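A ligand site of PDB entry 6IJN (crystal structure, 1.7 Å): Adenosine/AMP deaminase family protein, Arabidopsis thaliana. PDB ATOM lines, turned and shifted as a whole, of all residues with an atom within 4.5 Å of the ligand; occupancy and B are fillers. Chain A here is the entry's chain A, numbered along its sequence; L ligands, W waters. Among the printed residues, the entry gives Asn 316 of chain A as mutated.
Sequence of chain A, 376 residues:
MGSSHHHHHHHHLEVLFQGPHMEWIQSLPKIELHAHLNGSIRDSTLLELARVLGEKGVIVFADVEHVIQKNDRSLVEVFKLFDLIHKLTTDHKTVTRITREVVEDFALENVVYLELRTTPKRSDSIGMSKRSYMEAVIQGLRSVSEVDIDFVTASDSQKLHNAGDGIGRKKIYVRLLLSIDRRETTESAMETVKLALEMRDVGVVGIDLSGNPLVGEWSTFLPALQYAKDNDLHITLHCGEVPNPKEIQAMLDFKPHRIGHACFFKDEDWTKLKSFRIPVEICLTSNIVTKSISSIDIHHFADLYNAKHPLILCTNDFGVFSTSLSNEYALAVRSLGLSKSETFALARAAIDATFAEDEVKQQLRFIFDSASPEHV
NE2 of His 86 sits at hydrogen-bond distance from O7 of the ligand (2.7 Å). An oxygen (O2) of the ligand lies within hydrogen-bond range of the side-chain amide nitrogen of Asn 38 (2.9 Å). N of Thr 119 sits at hydrogen-bond distance from O1 of the ligand (2.7 Å). The side-chain hydroxyl (OG1) of Thr 118 sits at hydrogen-bond distance from an oxygen (O2) of the ligand (2.7 Å). The backbone NH (N) of Asn 38 is in hydrogen-bond range of an oxygen (O2) of the ligand. An oxygen (O7) of the ligand is in salt-bridge range of the side-chain amino group (NZ) of Lys 121. ND1 of His 36 is in hydrogen-bond range of O4 of the ligand, 3.0 Å away. The side-chain carboxylate (OD2) of Asp 317 is in hydrogen-bond range of a nitrogen (N5) of the ligand, at 2.7 Å. A nitrogen (N2) of the ligand lies within hydrogen-bond range of the backbone NH of Gly 211. The side-chain amide nitrogen of Asn 316 lies close to a nitrogen (N4) of the ligand (3.0 Å). The side-chain hydroxyl of Thr 119 is in hydrogen-bond range of an oxygen (O1) of the ligand, at 2.7 Å. The side-chain carboxylate (OE1) of Glu 241 lies within hydrogen-bond range of a nitrogen (N3) of the ligand (2.7 Å).
The backbone carbonyl oxygen of Asn 316 is in hydrogen-bond range of the backbone NH of His 36 (3.0 Å). OD2 of Asp 317 sits close to OD1 of Asn 316 (3.1 Å). The side-chain amide nitrogen of Asn 38 sits at hydrogen-bond distance from the side-chain hydroxyl of Tyr 133 (3.2 Å). The side-chain carboxylate of Asp 181 lies within salt-bridge range of the guanidinium group of Arg 183, 2.9 Å away. The side-chain hydroxyl (OG1) of Thr 118 is in hydrogen-bond range of the side-chain hydroxyl (OH) of Tyr 133. NZ of Lys 121 sits at hydrogen-bond distance from OH of Tyr 133, 3.1 Å away. A ring nitrogen (NE2) of His 36 sits at hydrogen-bond distance from a ring nitrogen (NE2) of His 238, 3.1 Å away. The side-chain amide nitrogen (ND2) of Asn 316 sits at hydrogen-bond distance from the side-chain hydroxyl (OG) of Ser 286, 2.8 Å away.
Residues that only touch the ligand: Leu 37 (3.5 Å), Val 78 (3.997 Å), Phe 79 (3.6 Å), Phe 82 (3.4 Å), Asp 181 (3.5 Å), Ser 210 (3.8 Å), His 238 (3.4 Å) and His 261 (3.6 Å). Hydrophobic or aromatic side chains that line the ligand: His 36, Leu 37, Val 78, Phe 79, Phe 82, His 86 and His 238. Within 4 Å of the ligand: His 36, Leu 37, Asn 38, Val 78, Phe 79, Phe 82, His 86, Thr 118, Thr 119, Lys 121, Asp 181, Ser 210, Gly 211, His 238, Glu 241, His 261, Asn 316 and Asp 317. The nearest printed residue that does not touch the ligand is Tyr 133 (4.02 Å).
Water W4 bridges O1 of the ligand (2.6 Å) and ND1 of His 36 (2.7 Å). Water W1 lies within hydrogen-bond range of the side-chain hydroxyl of Ser 210 (2.7 Å), an oxygen (O5) of the ligand (2.8 Å) and the side-chain hydroxyl of Thr 119 (2.8 Å). Water W5 bridges O6 of the ligand and NH1 of Arg 183. Water W2 lies within hydrogen-bond range of the side-chain amide oxygen (OD1) of Asn 316 (2.5 Å), a ring nitrogen (NE2) of His 238 (2.5 Å), a ring nitrogen (NE2) of His 261 (2.7 Å), a nitrogen (N4) of the ligand (3.0 Å) and a ring nitrogen (NE2) of His 36 (3.1 Å). Water W3 lies within hydrogen-bond range of OD1 of Asp 181 (2.7 Å), O6 of the ligand (2.9 Å) and OG1 of Thr 119 (3.1 Å).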
ATOM      1  N   HIS A  36     -22.998  18.529 -20.904  1.00  0.00           N
ATOM      2  CA  HIS A  36     -23.467  19.440 -21.934  1.00  0.00           C
ATOM      3  C   HIS A  36     -24.267  20.554 -21.276  1.00  0.00           C
ATOM      4  O   HIS A  36     -25.176  20.275 -20.480  1.00  0.00           O
ATOM      5  CB  HIS A  36     -24.376  18.721 -22.935  1.00  0.00           C
ATOM      6  CG  HIS A  36     -23.721  17.587 -23.678  1.00  0.00           C
ATOM      7  ND1 HIS A  36     -23.142  17.753 -24.919  1.00  0.00           N
ATOM      8  CD2 HIS A  36     -23.562  16.272 -23.351  1.00  0.00           C
ATOM      9  CE1 HIS A  36     -22.658  16.592 -25.342  1.00  0.00           C
ATOM     10  NE2 HIS A  36     -22.916  15.678 -24.415  1.00  0.00           N
ATOM     11  N   LEU A  37     -23.947  21.799 -21.618  1.00  0.00           N
ATOM     12  CA  LEU A  37     -24.566  22.950 -20.952  1.00  0.00           C
ATOM     13  C   LEU A  37     -26.088  22.854 -20.972  1.00  0.00           C
ATOM     14  O   LEU A  37     -26.737  22.920 -19.920  1.00  0.00           O
ATOM     15  CB  LEU A  37     -24.076  24.235 -21.635  1.00  0.00           C
ATOM     16  CG  LEU A  37     -24.768  25.503 -21.135  1.00  0.00           C
ATOM     17  CD1 LEU A  37     -24.479  25.683 -19.618  1.00  0.00           C
ATOM     18  CD2 LEU A  37     -24.224  26.663 -21.915  1.00  0.00           C
ATOM     19  N   ASN A  38     -26.697  22.705 -22.150  1.00  0.00           N
ATOM     20  CA  ASN A  38     -28.151  22.734 -22.181  1.00  0.00           C
ATOM     21  C   ASN A  38     -28.797  21.417 -21.757  1.00  0.00           C
ATOM     22  O   ASN A  38     -30.033  21.338 -21.729  1.00  0.00           O
ATOM     23  CB  ASN A  38     -28.651  23.163 -23.564  1.00  0.00           C
ATOM     24  CG  ASN A  38     -28.493  24.658 -23.801  1.00  0.00           C
ATOM     25  OD1 ASN A  38     -29.424  25.444 -23.554  1.00  0.00           O
ATOM     26  ND2 ASN A  38     -27.322  25.077 -24.268  1.00  0.00           N
ATOM     27  N   GLY A  39     -28.006  20.408 -21.426  1.00  0.00           N
ATOM     28  CA  GLY A  39     -28.507  19.217 -20.750  1.00  0.00           C
ATOM     29  C   GLY A  39     -28.380  19.256 -19.241  1.00  0.00           C
ATOM     30  O   GLY A  39     -28.709  18.280 -18.582  1.00  0.00           O
ATOM     31  N   VAL A  78     -34.816  11.708 -26.481  1.00  0.00           N
ATOM     32  CA  VAL A  78     -33.874  12.672 -25.906  1.00  0.00           C
ATOM     33  C   VAL A  78     -33.598  13.817 -26.897  1.00  0.00           C
ATOM     34  O   VAL A  78     -33.519  14.992 -26.509  1.00  0.00           O
ATOM     35  CB  VAL A  78     -32.578  11.946 -25.455  1.00  0.00           C
ATOM     36  CG1 VAL A  78     -31.437  12.921 -25.327  1.00  0.00           C
ATOM     37  CG2 VAL A  78     -32.782  11.248 -24.119  1.00  0.00           C
ATOM     38  N   PHE A  79     -33.440  13.505 -28.188  1.00  0.00           N
ATOM     39  CA  PHE A  79     -33.110  14.573 -29.122  1.00  0.00           C
ATOM     40  C   PHE A  79     -34.321  15.444 -29.461  1.00  0.00           C
ATOM     41  O   PHE A  79     -34.164  16.640 -29.742  1.00  0.00           O
ATOM     42  CB  PHE A  79     -32.436  13.973 -30.371  1.00  0.00           C
ATOM     43  CG  PHE A  79     -31.120  13.343 -30.028  1.00  0.00           C
ATOM     44  CD1 PHE A  79     -30.014  14.147 -29.753  1.00  0.00           C
ATOM     45  CD2 PHE A  79     -31.042  11.982 -29.794  1.00  0.00           C
ATOM     46  CE1 PHE A  79     -28.824  13.582 -29.332  1.00  0.00           C
ATOM     47  CE2 PHE A  79     -29.855  11.411 -29.396  1.00  0.00           C
ATOM     48  CZ  PHE A  79     -28.745  12.216 -29.135  1.00  0.00           C
ATOM     49  N   PHE A  82     -34.150  17.882 -26.669  1.00  0.00           N
ATOM     50  CA  PHE A  82     -33.179  18.963 -26.890  1.00  0.00           C
ATOM     51  C   PHE A  82     -33.709  20.005 -27.854  1.00  0.00           C
ATOM     52  O   PHE A  82     -33.417  21.197 -27.695  1.00  0.00           O
ATOM     53  CB  PHE A  82     -31.855  18.399 -27.390  1.00  0.00           C
ATOM     54  CG  PHE A  82     -31.032  17.810 -26.295  1.00  0.00           C
ATOM     55  CD1 PHE A  82     -30.731  18.567 -25.162  1.00  0.00           C
ATOM     56  CD2 PHE A  82     -30.568  16.510 -26.394  1.00  0.00           C
ATOM     57  CE1 PHE A  82     -29.958  18.014 -24.135  1.00  0.00           C
ATOM     58  CE2 PHE A  82     -29.815  15.939 -25.360  1.00  0.00           C
ATOM     59  CZ  PHE A  82     -29.519  16.711 -24.256  1.00  0.00           C
ATOM     60  N   HIS A  86     -33.849  23.905 -26.699  1.00  0.00           N
ATOM     61  CA  HIS A  86     -33.199  24.974 -27.432  1.00  0.00           C
ATOM     62  C   HIS A  86     -34.177  26.057 -27.824  1.00  0.00           C
ATOM     63  O   HIS A  86     -33.778  27.221 -27.971  1.00  0.00           O
ATOM     64  CB  HIS A  86     -32.505  24.420 -28.669  1.00  0.00           C
ATOM     65  CG  HIS A  86     -31.276  23.613 -28.362  1.00  0.00           C
ATOM     66  ND1 HIS A  86     -30.826  22.599 -29.182  1.00  0.00           N
ATOM     67  CD2 HIS A  86     -30.412  23.678 -27.319  1.00  0.00           C
ATOM     68  CE1 HIS A  86     -29.731  22.070 -28.649  1.00  0.00           C
ATOM     69  NE2 HIS A  86     -29.459  22.698 -27.517  1.00  0.00           N
ATOM     70  N   ARG A 117     -19.116  21.512 -21.954  1.00  0.00           N
ATOM     71  CA  ARG A 117     -19.182  21.528 -23.404  1.00  0.00           C
ATOM     72  C   ARG A 117     -20.507  22.115 -23.858  1.00  0.00           C
ATOM     73  O   ARG A 117     -21.518  21.989 -23.181  1.00  0.00           O
ATOM     74  CB  ARG A 117     -18.983  20.120 -23.975  1.00  0.00           C
ATOM     75  CG  ARG A 117     -20.046  19.127 -23.584  1.00  0.00           C
ATOM     76  CD  ARG A 117     -19.672  17.776 -24.199  1.00  0.00           C
ATOM     77  NE  ARG A 117     -18.518  17.187 -23.525  1.00  0.00           N
ATOM     78  CZ  ARG A 117     -17.931  16.070 -23.916  1.00  0.00           C
ATOM     79  NH1 ARG A 117     -18.277  15.473 -25.056  1.00  0.00           N
ATOM     80  NH2 ARG A 117     -16.959  15.546 -23.179  1.00  0.00           N
ATOM     81  N   THR A 118     -20.469  22.833 -24.984  1.00  0.00           N
ATOM     82  CA  THR A 118     -21.739  23.360 -25.497  1.00  0.00           C
ATOM     83  C   THR A 118     -21.598  23.590 -26.985  1.00  0.00           C
ATOM     84  O   THR A 118     -20.506  23.878 -27.459  1.00  0.00           O
ATOM     85  CB  THR A 118     -22.169  24.653 -24.779  1.00  0.00           C
ATOM     86  OG1 THR A 118     -23.509  25.028 -25.166  1.00  0.00           O
ATOM     87  CG2 THR A 118     -21.223  25.808 -25.063  1.00  0.00           C
ATOM     88  N   THR A 119     -22.706  23.405 -27.709  1.00  0.00           N
ATOM     89  CA  THR A 119     -22.786  23.675 -29.140  1.00  0.00           C
ATOM     90  C   THR A 119     -23.017  25.156 -29.363  1.00  0.00           C
ATOM     91  O   THR A 119     -24.083  25.666 -28.993  1.00  0.00           O
ATOM     92  CB  THR A 119     -23.965  22.921 -29.752  1.00  0.00           C
ATOM     93  OG1 THR A 119     -23.998  21.571 -29.296  1.00  0.00           O
ATOM     94  CG2 THR A 119     -23.873  22.960 -31.291  1.00  0.00           C
ATOM     95  N   LYS A 121     -24.443  28.273 -31.073  1.00  0.00           N
ATOM     96  CA  LYS A 121     -25.622  28.381 -31.914  1.00  0.00           C
ATOM     97  C   LYS A 121     -25.586  29.663 -32.731  1.00  0.00           C
ATOM     98  O   LYS A 121     -25.064  30.692 -32.295  1.00  0.00           O
ATOM     99  CB  LYS A 121     -26.925  28.365 -31.109  1.00  0.00           C
ATOM    100  CG  LYS A 121     -27.052  27.342 -29.977  1.00  0.00           C
ATOM    101  CD  LYS A 121     -27.100  25.935 -30.473  1.00  0.00           C
ATOM    102  CE  LYS A 121     -27.505  24.954 -29.319  1.00  0.00           C
ATOM    103  NZ  LYS A 121     -26.723  25.229 -28.037  1.00  0.00           N
ATOM    104  N   TYR A 133     -22.778  33.682 -29.031  1.00  0.00           N
ATOM    105  CA  TYR A 133     -23.217  32.659 -28.105  1.00  0.00           C
ATOM    106  C   TYR A 133     -22.090  32.312 -27.122  1.00  0.00           C
ATOM    107  O   TYR A 133     -22.291  32.264 -25.900  1.00  0.00           O
ATOM    108  CB  TYR A 133     -23.672  31.422 -28.901  1.00  0.00           C
ATOM    109  CG  TYR A 133     -24.119  30.242 -28.076  1.00  0.00           C
ATOM    110  CD1 TYR A 133     -25.451  29.924 -27.941  1.00  0.00           C
ATOM    111  CD2 TYR A 133     -23.177  29.423 -27.449  1.00  0.00           C
ATOM    112  CE1 TYR A 133     -25.855  28.811 -27.186  1.00  0.00           C
ATOM    113  CE2 TYR A 133     -23.551  28.320 -26.721  1.00  0.00           C
ATOM    114  CZ  TYR A 133     -24.886  28.014 -26.592  1.00  0.00           C
ATOM    115  OH  TYR A 133     -25.236  26.900 -25.882  1.00  0.00           O
ATOM    116  N   ASP A 181     -22.337  19.625 -33.654  1.00  0.00           N
ATOM    117  CA  ASP A 181     -23.542  18.819 -33.704  1.00  0.00           C
ATOM    118  C   ASP A 181     -23.548  18.053 -35.026  1.00  0.00           C
ATOM    119  O   ASP A 181     -23.210  18.608 -36.071  1.00  0.00           O
ATOM    120  CB  ASP A 181     -24.730  19.781 -33.585  1.00  0.00           C
ATOM    121  CG  ASP A 181     -26.084  19.089 -33.522  1.00  0.00           C
ATOM    122  OD1 ASP A 181     -26.880  19.431 -32.615  1.00  0.00           O
ATOM    123  OD2 ASP A 181     -26.397  18.261 -34.379  1.00  0.00           O
ATOM    124  N   ARG A 183     -25.705  17.273 -36.971  1.00  0.00           N
ATOM    125  CA  ARG A 183     -26.539  17.857 -38.025  1.00  0.00           C
ATOM    126  C   ARG A 183     -25.829  18.904 -38.870  1.00  0.00           C
ATOM    127  O   ARG A 183     -26.409  19.376 -39.864  1.00  0.00           O
ATOM    128  CB  ARG A 183     -27.781  18.492 -37.392  1.00  0.00           C
ATOM    129  CG  ARG A 183     -28.697  17.481 -36.737  1.00  0.00           C
ATOM    130  CD  ARG A 183     -29.838  18.208 -36.059  1.00  0.00           C
ATOM    131  NE  ARG A 183     -29.397  18.849 -34.823  1.00  0.00           N
ATOM    132  CZ  ARG A 183     -30.211  19.479 -33.983  1.00  0.00           C
ATOM    133  NH1 ARG A 183     -29.747  19.957 -32.833  1.00  0.00           N
ATOM    134  NH2 ARG A 183     -31.502  19.614 -34.312  1.00  0.00           N
ATOM    135  N   SER A 210     -20.832  15.589 -31.134  1.00  0.00           N
ATOM    136  CA  SER A 210     -21.975  15.053 -30.401  1.00  0.00           C
ATOM    137  C   SER A 210     -23.224  15.331 -31.232  1.00  0.00           C
ATOM    138  O   SER A 210     -23.134  15.644 -32.423  1.00  0.00           O
ATOM    139  CB  SER A 210     -22.057  15.653 -28.983  1.00  0.00           C
ATOM    140  OG  SER A 210     -22.014  17.073 -29.038  1.00  0.00           O
ATOM    141  N   GLY A 211     -24.393  15.216 -30.625  1.00  0.00           N
ATOM    142  CA  GLY A 211     -25.640  15.304 -31.346  1.00  0.00           C
ATOM    143  C   GLY A 211     -26.143  13.925 -31.708  1.00  0.00           C
ATOM    144  O   GLY A 211     -25.577  12.899 -31.343  1.00  0.00           O
ATOM    145  N   HIS A 238     -18.137  11.602 -29.144  1.00  0.00           N
ATOM    146  CA  HIS A 238     -19.180  10.623 -28.797  1.00  0.00           C
ATOM    147  C   HIS A 238     -19.067   9.450 -29.761  1.00  0.00           C
ATOM    148  O   HIS A 238     -19.117   9.633 -30.981  1.00  0.00           O
ATOM    149  CB  HIS A 238     -20.578  11.242 -28.928  1.00  0.00           C
ATOM    150  CG  HIS A 238     -20.959  12.171 -27.814  1.00  0.00           C
ATOM    151  ND1 HIS A 238     -20.066  13.046 -27.219  1.00  0.00           N
ATOM    152  CD2 HIS A 238     -22.160  12.410 -27.225  1.00  0.00           C
ATOM    153  CE1 HIS A 238     -20.692  13.762 -26.304  1.00  0.00           C
ATOM    154  NE2 HIS A 238     -21.961  13.405 -26.296  1.00  0.00           N
ATOM    155  N   GLU A 241     -22.651   5.289 -29.597  1.00  0.00           N
ATOM    156  CA  GLU A 241     -23.932   5.420 -28.902  1.00  0.00           C
ATOM    157  C   GLU A 241     -24.998   4.495 -29.490  1.00  0.00           C
ATOM    158  O   GLU A 241     -25.948   4.121 -28.775  1.00  0.00           O
ATOM    159  CB  GLU A 241     -24.432   6.854 -28.988  1.00  0.00           C
ATOM    160  CG  GLU A 241     -23.764   7.771 -28.012  1.00  0.00           C
ATOM    161  CD  GLU A 241     -24.318   9.168 -28.146  1.00  0.00           C
ATOM    162  OE1 GLU A 241     -25.319   9.481 -27.480  1.00  0.00           O
ATOM    163  OE2 GLU A 241     -23.761   9.923 -28.955  1.00  0.00           O
ATOM    164  N   HIS A 261     -19.177   7.551 -24.041  1.00  0.00           N
ATOM    165  CA  HIS A 261     -20.235   6.531 -24.145  1.00  0.00           C
ATOM    166  C   HIS A 261     -19.676   5.135 -24.429  1.00  0.00           C
ATOM    167  O   HIS A 261     -19.510   4.358 -23.485  1.00  0.00           O
ATOM    168  CB  HIS A 261     -21.300   6.926 -25.164  1.00  0.00           C
ATOM    169  CG  HIS A 261     -22.169   8.058 -24.698  1.00  0.00           C
ATOM    170  ND1 HIS A 261     -22.979   7.971 -23.574  1.00  0.00           N
ATOM    171  CD2 HIS A 261     -22.318   9.321 -25.161  1.00  0.00           C
ATOM    172  CE1 HIS A 261     -23.592   9.122 -23.384  1.00  0.00           C
ATOM    173  NE2 HIS A 261     -23.228   9.956 -24.345  1.00  0.00           N
ATOM    174  N   SER A 286     -27.337   8.066 -17.839  1.00  0.00           N
ATOM    175  CA  SER A 286     -27.718   8.276 -19.224  1.00  0.00           C
ATOM    176  C   SER A 286     -27.864   6.953 -19.986  1.00  0.00           C
ATOM    177  O   SER A 286     -28.891   6.705 -20.631  1.00  0.00           O
ATOM    178  CB  SER A 286     -26.652   9.148 -19.893  1.00  0.00           C
ATOM    179  OG  SER A 286     -26.957   9.374 -21.249  1.00  0.00           O
ATOM    180  N   ASN A 316     -23.036  13.533 -18.212  1.00  0.00           N
ATOM    181  CA  ASN A 316     -23.593  13.719 -19.557  1.00  0.00           C
ATOM    182  C   ASN A 316     -24.602  14.865 -19.597  1.00  0.00           C
ATOM    183  O   ASN A 316     -24.311  15.914 -20.168  1.00  0.00           O
ATOM    184  CB  ASN A 316     -24.209  12.422 -20.093  1.00  0.00           C
ATOM    185  CG  ASN A 316     -24.676  12.547 -21.518  1.00  0.00           C
ATOM    186  OD1 ASN A 316     -24.197  13.405 -22.269  1.00  0.00           O
ATOM    187  ND2 ASN A 316     -25.632  11.707 -21.890  1.00  0.00           N
ATOM    188  N   ASP A 317     -25.794  14.674 -19.005  1.00  0.00           N
ATOM    189  CA  ASP A 317     -26.843  15.704 -18.988  1.00  0.00           C
ATOM    190  C   ASP A 317     -27.566  15.581 -17.639  1.00  0.00           C
ATOM    191  O   ASP A 317     -28.583  14.895 -17.561  1.00  0.00           O
ATOM    192  CB  ASP A 317     -27.848  15.538 -20.124  1.00  0.00           C
ATOM    193  CG  ASP A 317     -27.234  15.569 -21.512  1.00  0.00           C
ATOM    194  OD1 ASP A 317     -26.913  16.662 -21.997  1.00  0.00           O
ATOM    195  OD2 ASP A 317     -27.142  14.491 -22.146  1.00  0.00           O
ATOM    196  N   PHE A 321     -31.341  13.919 -17.251  1.00  0.00           N
ATOM    197  CA  PHE A 321     -31.403  12.602 -16.651  1.00  0.00           C
ATOM    198  C   PHE A 321     -31.556  12.636 -15.142  1.00  0.00           C
ATOM    199  O   PHE A 321     -31.481  11.580 -14.505  1.00  0.00           O
ATOM    200  CB  PHE A 321     -30.193  11.762 -17.052  1.00  0.00           C
ATOM    201  CG  PHE A 321     -30.160  11.471 -18.513  1.00  0.00           C
ATOM    202  CD1 PHE A 321     -31.093  10.617 -19.080  1.00  0.00           C
ATOM    203  CD2 PHE A 321     -29.242  12.110 -19.337  1.00  0.00           C
ATOM    204  CE1 PHE A 321     -31.086  10.374 -20.431  1.00  0.00           C
ATOM    205  CE2 PHE A 321     -29.230  11.865 -20.680  1.00  0.00           C
ATOM    206  CZ  PHE A 321     -30.168  11.000 -21.235  1.00  0.00           C
HETATM  207  C1  LIG L   1     -25.370  12.895 -28.089  1.00  0.00           C
HETATM  208  C2  LIG L   1     -25.822  14.743 -26.781  1.00  0.00           C
HETATM  209  C3  LIG L   1     -26.134  13.991 -25.738  1.00  0.00           C
HETATM  210  O1  LIG L   1     -24.610  21.776 -26.717  1.00  0.00           O
HETATM  211  O2  LIG L   1     -25.310  23.065 -24.679  1.00  0.00           O
HETATM  212  N1  LIG L   1     -25.933  16.031 -26.444  1.00  0.00           N
HETATM  213  N2  LIG L   1     -25.438  14.240 -27.954  1.00  0.00           N
HETATM  214  N3  LIG L   1     -25.678  12.091 -27.036  1.00  0.00           N
HETATM  215  C4  LIG L   1     -26.052  12.627 -25.886  1.00  0.00           C
HETATM  216  N4  LIG L   1     -26.363  11.711 -24.833  1.00  0.00           N
HETATM  217  C5  LIG L   1     -27.791  11.460 -24.589  1.00  0.00           C
HETATM  218  N5  LIG L   1     -26.461  14.814 -24.703  1.00  0.00           N
HETATM  219  C6  LIG L   1     -26.346  16.092 -25.154  1.00  0.00           C
HETATM  220  O3  LIG L   1     -26.335  20.927 -25.106  1.00  0.00           O
HETATM  221  C7  LIG L   1     -27.263  20.053 -25.740  1.00  0.00           C
HETATM  222  C8  LIG L   1     -26.667  19.309 -26.916  1.00  0.00           C
HETATM  223  O4  LIG L   1     -25.686  18.369 -26.469  1.00  0.00           O
HETATM  224  C9  LIG L   1     -25.719  17.203 -27.286  1.00  0.00           C
HETATM  225  C10 LIG L   1     -26.861  17.363 -28.302  1.00  0.00           C
HETATM  226  O5  LIG L   1     -26.309  17.767 -29.544  1.00  0.00           O
HETATM  227  C11 LIG L   1     -27.692  18.466 -27.675  1.00  0.00           C
HETATM  228  O6  LIG L   1     -28.419  19.234 -28.620  1.00  0.00           O
HETATM  229  P1  LIG L   1     -25.769  22.223 -25.856  1.00  0.00           P
HETATM  230  O7  LIG L   1     -26.921  22.829 -26.645  1.00  0.00           O
HETATM  231  O   HOH W   1     -23.782  18.821 -29.971  1.00  0.00           O
HETATM  232  O   HOH W   2     -23.560  12.626 -24.520  1.00  0.00           O
HETATM  233  O   HOH W   3     -26.816  20.889 -30.328  1.00  0.00           O
HETATM  234  O   HOH W   4     -22.692  20.151 -26.047  1.00  0.00           O
HETATM  235  O   HOH W   5     -29.506  17.430 -30.510  1.00  0.00           O
